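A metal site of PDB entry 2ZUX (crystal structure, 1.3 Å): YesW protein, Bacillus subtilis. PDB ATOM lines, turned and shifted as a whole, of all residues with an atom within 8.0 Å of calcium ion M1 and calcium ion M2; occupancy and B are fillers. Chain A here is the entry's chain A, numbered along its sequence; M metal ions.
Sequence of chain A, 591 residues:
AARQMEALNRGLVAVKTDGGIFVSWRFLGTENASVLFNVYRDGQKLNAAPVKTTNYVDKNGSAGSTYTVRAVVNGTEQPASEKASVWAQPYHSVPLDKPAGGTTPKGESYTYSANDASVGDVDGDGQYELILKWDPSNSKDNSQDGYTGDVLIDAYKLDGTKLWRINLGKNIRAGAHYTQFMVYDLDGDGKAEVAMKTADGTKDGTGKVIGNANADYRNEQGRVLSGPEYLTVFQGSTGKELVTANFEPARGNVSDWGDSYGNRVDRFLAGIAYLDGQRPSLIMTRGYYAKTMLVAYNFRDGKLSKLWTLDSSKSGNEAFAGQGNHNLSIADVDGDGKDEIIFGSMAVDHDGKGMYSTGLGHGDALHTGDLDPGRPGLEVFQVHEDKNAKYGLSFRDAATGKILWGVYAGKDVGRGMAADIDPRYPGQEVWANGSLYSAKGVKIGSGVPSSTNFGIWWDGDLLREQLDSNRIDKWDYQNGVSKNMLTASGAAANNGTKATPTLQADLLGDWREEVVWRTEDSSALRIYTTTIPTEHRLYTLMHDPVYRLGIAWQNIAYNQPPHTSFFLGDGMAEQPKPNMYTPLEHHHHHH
The side-chain sulfur (SD) of Met 355 lies close to the backbone NH (N) of Asp 349 (3.5 Å). O of Ala 331 is in hydrogen-bond range of N of Glu 340 (2.8 Å). The backbone NH of Gly 337 lies within hydrogen-bond range of the side-chain carboxylate of Asp 332 (2.8 Å). The side-chain carboxylate (OD1) of Asp 332 lies close to the backbone NH (N) of Gly 335, 3.0 Å away. The backbone NH of Asp 332 lies within hydrogen-bond range of the side-chain carboxylate of Asp 339 (3.3 Å). The side-chain carboxylate (OE1) of Glu 340 sits close to the backbone NH (N) of Val 333 (2.9 Å).
Five residues have an atom within 4 Å of calcium ion M1: Asp 332, Asp 334, Asp 336, Lys 338 and Glu 340. The nearest printed residue that does not touch calcium ion M1 is Val 333 (4.1 Å).
Of the 20 residues printed, 5 come within 4 Å of calcium ion M2. The nearest printed residue that does not touch calcium ion M2 is Lys 338 (4.9 Å).
Calcium ion M1 is bound by OD1 of Asp 336 (2.1 Å), OD1 of Asp 334 (2.1 Å), O of Lys 338 (2.2 Å), OE2 of Glu 340 (2.3 Å), OD1 of Asp 332 (2.3 Å) and OE1 of Glu 340 (2.4 Å). Calcium ion M1 has six donor atoms within binding distance.
Calcium ion M2 is bound by OD1 of Asp 349 (2.4 Å), OE2 of Glu 340 (2.4 Å), OD2 of Asp 336 (2.4 Å), OD2 of Asp 334 (2.4 Å) and ND1 of His 350 (2.6 Å).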
ATOM      1  N   ARG A   3      -7.728   1.757 -13.816  1.00  0.00           N
ATOM      2  CA  ARG A   3      -7.105   0.454 -14.110  1.00  0.00           C
ATOM      3  C   ARG A   3      -8.129  -0.632 -14.362  1.00  0.00           C
ATOM      4  O   ARG A   3      -9.163  -0.691 -13.689  1.00  0.00           O
ATOM      5  CB  ARG A   3      -6.260  -0.014 -12.924  1.00  0.00           C
ATOM      6  CG  ARG A   3      -5.017   0.750 -12.703  1.00  0.00           C
ATOM      7  CD  ARG A   3      -4.148   0.029 -11.705  1.00  0.00           C
ATOM      8  NE  ARG A   3      -2.883   0.714 -11.595  1.00  0.00           N
ATOM      9  CZ  ARG A   3      -1.751   0.130 -11.244  1.00  0.00           C
ATOM     10  NH1 ARG A   3      -1.718  -1.160 -10.940  1.00  0.00           N
ATOM     11  NH2 ARG A   3      -0.652   0.858 -11.197  1.00  0.00           N
ATOM     12  N   TYR A 274       1.116  -3.252 -14.051  1.00  0.00           N
ATOM     13  CA  TYR A 274       0.432  -2.345 -14.975  1.00  0.00           C
ATOM     14  C   TYR A 274       1.431  -1.289 -15.456  1.00  0.00           C
ATOM     15  O   TYR A 274       1.405  -0.128 -15.015  1.00  0.00           O
ATOM     16  CB  TYR A 274      -0.788  -1.699 -14.301  1.00  0.00           C
ATOM     17  CG  TYR A 274      -1.974  -2.631 -14.139  1.00  0.00           C
ATOM     18  CD1 TYR A 274      -3.232  -2.278 -14.642  1.00  0.00           C
ATOM     19  CD2 TYR A 274      -1.839  -3.871 -13.507  1.00  0.00           C
ATOM     20  CE1 TYR A 274      -4.322  -3.137 -14.500  1.00  0.00           C
ATOM     21  CE2 TYR A 274      -2.932  -4.730 -13.356  1.00  0.00           C
ATOM     22  CZ  TYR A 274      -4.167  -4.353 -13.860  1.00  0.00           C
ATOM     23  OH  TYR A 274      -5.238  -5.197 -13.723  1.00  0.00           O
ATOM     24  N   LEU A 275       2.311  -1.709 -16.360  1.00  0.00           N
ATOM     25  CA  LEU A 275       3.389  -0.867 -16.852  1.00  0.00           C
ATOM     26  C   LEU A 275       2.899   0.351 -17.621  1.00  0.00           C
ATOM     27  O   LEU A 275       3.564   1.401 -17.622  1.00  0.00           O
ATOM     28  CB  LEU A 275       4.343  -1.681 -17.721  1.00  0.00           C
ATOM     29  CG  LEU A 275       4.939  -2.937 -17.056  1.00  0.00           C
ATOM     30  CD1 LEU A 275       5.678  -3.759 -18.089  1.00  0.00           C
ATOM     31  CD2 LEU A 275       5.848  -2.567 -15.891  1.00  0.00           C
ATOM     32  N   GLY A 277      -0.079   1.728 -16.908  1.00  0.00           N
ATOM     33  CA  GLY A 277      -0.965   2.429 -15.978  1.00  0.00           C
ATOM     34  C   GLY A 277      -2.442   2.107 -16.126  1.00  0.00           C
ATOM     35  O   GLY A 277      -3.267   2.639 -15.381  1.00  0.00           O
ATOM     36  N   ALA A 331       4.316  -2.134  -7.461  1.00  0.00           N
ATOM     37  CA  ALA A 331       3.527  -1.021  -6.984  1.00  0.00           C
ATOM     38  C   ALA A 331       3.865   0.227  -7.768  1.00  0.00           C
ATOM     39  O   ALA A 331       4.987   0.385  -8.254  1.00  0.00           O
ATOM     40  CB  ALA A 331       3.783  -0.766  -5.497  1.00  0.00           C
ATOM     41  N   ASP A 332       2.910   1.144  -7.844  1.00  0.00           N
ATOM     42  CA  ASP A 332       3.188   2.472  -8.361  1.00  0.00           C
ATOM     43  C   ASP A 332       3.825   3.260  -7.222  1.00  0.00           C
ATOM     44  O   ASP A 332       3.133   3.723  -6.309  1.00  0.00           O
ATOM     45  CB  ASP A 332       1.912   3.147  -8.851  1.00  0.00           C
ATOM     46  CG  ASP A 332       2.135   4.583  -9.290  1.00  0.00           C
ATOM     47  OD1 ASP A 332       3.297   4.972  -9.535  1.00  0.00           O
ATOM     48  OD2 ASP A 332       1.146   5.332  -9.390  1.00  0.00           O
ATOM     49  N   VAL A 333       5.144   3.393  -7.276  1.00  0.00           N
ATOM     50  CA  VAL A 333       5.887   4.027  -6.190  1.00  0.00           C
ATOM     51  C   VAL A 333       6.152   5.505  -6.446  1.00  0.00           C
ATOM     52  O   VAL A 333       6.382   6.259  -5.512  1.00  0.00           O
ATOM     53  CB  VAL A 333       7.244   3.318  -5.896  1.00  0.00           C
ATOM     54  CG1 VAL A 333       7.021   1.841  -5.553  1.00  0.00           C
ATOM     55  CG2 VAL A 333       8.229   3.476  -7.077  1.00  0.00           C
ATOM     56  N   ASP A 334       6.128   5.918  -7.715  1.00  0.00           N
ATOM     57  CA  ASP A 334       6.512   7.279  -8.082  1.00  0.00           C
ATOM     58  C   ASP A 334       5.330   8.178  -8.441  1.00  0.00           C
ATOM     59  O   ASP A 334       5.518   9.352  -8.782  1.00  0.00           O
ATOM     60  CB  ASP A 334       7.595   7.277  -9.183  1.00  0.00           C
ATOM     61  CG  ASP A 334       7.131   6.581 -10.454  1.00  0.00           C
ATOM     62  OD1 ASP A 334       5.930   6.308 -10.575  1.00  0.00           O
ATOM     63  OD2 ASP A 334       7.988   6.308 -11.330  1.00  0.00           O
ATOM     64  N   GLY A 335       4.117   7.640  -8.362  1.00  0.00           N
ATOM     65  CA  GLY A 335       2.883   8.409  -8.521  1.00  0.00           C
ATOM     66  C   GLY A 335       2.424   8.691  -9.934  1.00  0.00           C
ATOM     67  O   GLY A 335       1.504   9.503 -10.126  1.00  0.00           O
ATOM     68  N   ASP A 336       3.028   8.049 -10.932  1.00  0.00           N
ATOM     69  CA  ASP A 336       2.652   8.274 -12.330  1.00  0.00           C
ATOM     70  C   ASP A 336       1.518   7.357 -12.824  1.00  0.00           C
ATOM     71  O   ASP A 336       1.152   7.393 -14.014  1.00  0.00           O
ATOM     72  CB  ASP A 336       3.886   8.195 -13.258  1.00  0.00           C
ATOM     73  CG  ASP A 336       4.552   6.821 -13.278  1.00  0.00           C
ATOM     74  OD1 ASP A 336       3.958   5.862 -12.716  1.00  0.00           O
ATOM     75  OD2 ASP A 336       5.662   6.679 -13.827  1.00  0.00           O
ATOM     76  N   GLY A 337       0.963   6.538 -11.931  1.00  0.00           N
ATOM     77  CA  GLY A 337      -0.125   5.610 -12.263  1.00  0.00           C
ATOM     78  C   GLY A 337       0.345   4.262 -12.787  1.00  0.00           C
ATOM     79  O   GLY A 337      -0.425   3.300 -12.870  1.00  0.00           O
ATOM     80  N   LYS A 338       1.618   4.210 -13.144  1.00  0.00           N
ATOM     81  CA  LYS A 338       2.236   3.033 -13.752  1.00  0.00           C
ATOM     82  C   LYS A 338       3.021   2.262 -12.699  1.00  0.00           C
ATOM     83  O   LYS A 338       3.623   2.852 -11.806  1.00  0.00           O
ATOM     84  CB  LYS A 338       3.157   3.460 -14.885  1.00  0.00           C
ATOM     85  CG  LYS A 338       2.441   4.311 -15.935  1.00  0.00           C
ATOM     86  CD  LYS A 338       3.385   4.775 -17.017  1.00  0.00           C
ATOM     87  CE  LYS A 338       2.652   5.621 -18.052  1.00  0.00           C
ATOM     88  NZ  LYS A 338       2.206   6.930 -17.480  1.00  0.00           N
ATOM     89  N   ASP A 339       3.013   0.932 -12.798  1.00  0.00           N
ATOM     90  CA  ASP A 339       3.699   0.101 -11.809  1.00  0.00           C
ATOM     91  C   ASP A 339       5.192  -0.005 -12.034  1.00  0.00           C
ATOM     92  O   ASP A 339       5.668  -0.153 -13.156  1.00  0.00           O
ATOM     93  CB  ASP A 339       3.093  -1.304 -11.777  1.00  0.00           C
ATOM     94  CG  ASP A 339       1.734  -1.349 -11.134  1.00  0.00           C
ATOM     95  OD1 ASP A 339       1.459  -0.505 -10.245  1.00  0.00           O
ATOM     96  OD2 ASP A 339       0.923  -2.205 -11.522  1.00  0.00           O
ATOM     97  N   GLU A 340       5.908   0.080 -10.918  1.00  0.00           N
ATOM     98  CA  GLU A 340       7.325  -0.225 -10.857  1.00  0.00           C
ATOM     99  C   GLU A 340       7.506  -1.570 -10.160  1.00  0.00           C
ATOM    100  O   GLU A 340       6.564  -2.121  -9.574  1.00  0.00           O
ATOM    101  CB  GLU A 340       8.047   0.893 -10.102  1.00  0.00           C
ATOM    102  CG  GLU A 340       8.201   2.197 -10.913  1.00  0.00           C
ATOM    103  CD  GLU A 340       6.909   3.021 -10.994  1.00  0.00           C
ATOM    104  OE1 GLU A 340       6.200   3.168  -9.968  1.00  0.00           O
ATOM    105  OE2 GLU A 340       6.571   3.524 -12.110  1.00  0.00           O
ATOM    106  N   ILE A 341       8.720  -2.098 -10.244  1.00  0.00           N
ATOM    107  CA  ILE A 341       9.043  -3.420  -9.710  1.00  0.00           C
ATOM    108  C   ILE A 341      10.067  -3.253  -8.587  1.00  0.00           C
ATOM    109  O   ILE A 341      11.146  -2.681  -8.813  1.00  0.00           O
ATOM    110  CB  ILE A 341       9.625  -4.332 -10.807  1.00  0.00           C
ATOM    111  CG1 ILE A 341       8.628  -4.493 -11.973  1.00  0.00           C
ATOM    112  CG2 ILE A 341      10.008  -5.695 -10.234  1.00  0.00           C
ATOM    113  CD1 ILE A 341       9.266  -4.814 -13.310  1.00  0.00           C
ATOM    114  N   VAL A 348      13.035  -1.299 -10.544  1.00  0.00           N
ATOM    115  CA  VAL A 348      13.007  -1.173 -11.990  1.00  0.00           C
ATOM    116  C   VAL A 348      11.764  -0.389 -12.361  1.00  0.00           C
ATOM    117  O   VAL A 348      10.676  -0.662 -11.857  1.00  0.00           O
ATOM    118  CB  VAL A 348      12.990  -2.564 -12.661  1.00  0.00           C
ATOM    119  CG1 VAL A 348      12.942  -2.462 -14.188  1.00  0.00           C
ATOM    120  CG2 VAL A 348      14.190  -3.387 -12.210  1.00  0.00           C
ATOM    121  N   ASP A 349      11.947   0.599 -13.244  1.00  0.00           N
ATOM    122  CA  ASP A 349      10.858   1.482 -13.668  1.00  0.00           C
ATOM    123  C   ASP A 349       9.903   0.771 -14.625  1.00  0.00           C
ATOM    124  O   ASP A 349      10.207  -0.305 -15.142  1.00  0.00           O
ATOM    125  CB  ASP A 349      11.461   2.733 -14.314  1.00  0.00           C
ATOM    126  CG  ASP A 349      10.615   3.969 -14.136  1.00  0.00           C
ATOM    127  OD1 ASP A 349       9.484   3.904 -13.598  1.00  0.00           O
ATOM    128  OD2 ASP A 349      11.102   5.046 -14.550  1.00  0.00           O
ATOM    129  N   HIS A 350       8.771   1.418 -14.890  1.00  0.00           N
ATOM    130  CA  HIS A 350       7.719   0.836 -15.717  1.00  0.00           C
ATOM    131  C   HIS A 350       8.168   0.584 -17.155  1.00  0.00           C
ATOM    132  O   HIS A 350       7.540  -0.196 -17.871  1.00  0.00           O
ATOM    133  CB  HIS A 350       6.497   1.748 -15.710  1.00  0.00           C
ATOM    134  CG  HIS A 350       6.699   3.042 -16.432  1.00  0.00           C
ATOM    135  ND1 HIS A 350       7.092   4.202 -15.803  1.00  0.00           N
ATOM    136  CD2 HIS A 350       6.598   3.351 -17.750  1.00  0.00           C
ATOM    137  CE1 HIS A 350       7.213   5.173 -16.696  1.00  0.00           C
ATOM    138  NE2 HIS A 350       6.914   4.671 -17.888  1.00  0.00           N
ATOM    139  N   ASP A 351       9.239   1.254 -17.581  1.00  0.00           N
ATOM    140  CA  ASP A 351       9.799   1.117 -18.917  1.00  0.00           C
ATOM    141  C   ASP A 351      11.037   0.214 -18.961  1.00  0.00           C
ATOM    142  O   ASP A 351      11.734   0.146 -19.978  1.00  0.00           O
ATOM    143  CB  ASP A 351      10.139   2.494 -19.487  1.00  0.00           C
ATOM    144  CG  ASP A 351      11.193   3.220 -18.677  1.00  0.00           C
ATOM    145  OD1 ASP A 351      11.616   2.722 -17.607  1.00  0.00           O
ATOM    146  OD2 ASP A 351      11.612   4.315 -19.103  1.00  0.00           O
ATOM    147  N   MET A 355      16.111   1.863 -11.658  1.00  0.00           N
ATOM    148  CA  MET A 355      15.878   3.104 -10.914  1.00  0.00           C
ATOM    149  C   MET A 355      16.957   3.392  -9.865  1.00  0.00           C
ATOM    150  O   MET A 355      17.525   4.485  -9.822  1.00  0.00           O
ATOM    151  CB  MET A 355      14.523   3.082 -10.216  1.00  0.00           C
ATOM    152  CG  MET A 355      13.360   3.044 -11.181  1.00  0.00           C
ATOM    153  SD  MET A 355      11.793   2.646 -10.383  1.00  0.00           S
ATOM    154  CE  MET A 355      11.519   4.089  -9.363  1.00  0.00           C
HETATM  155 CA    CA M   1       4.797   4.609 -11.215  1.00  0.00          CA
HETATM  156 CA    CA M   2       7.532   5.209 -13.460  1.00  0.00          CA
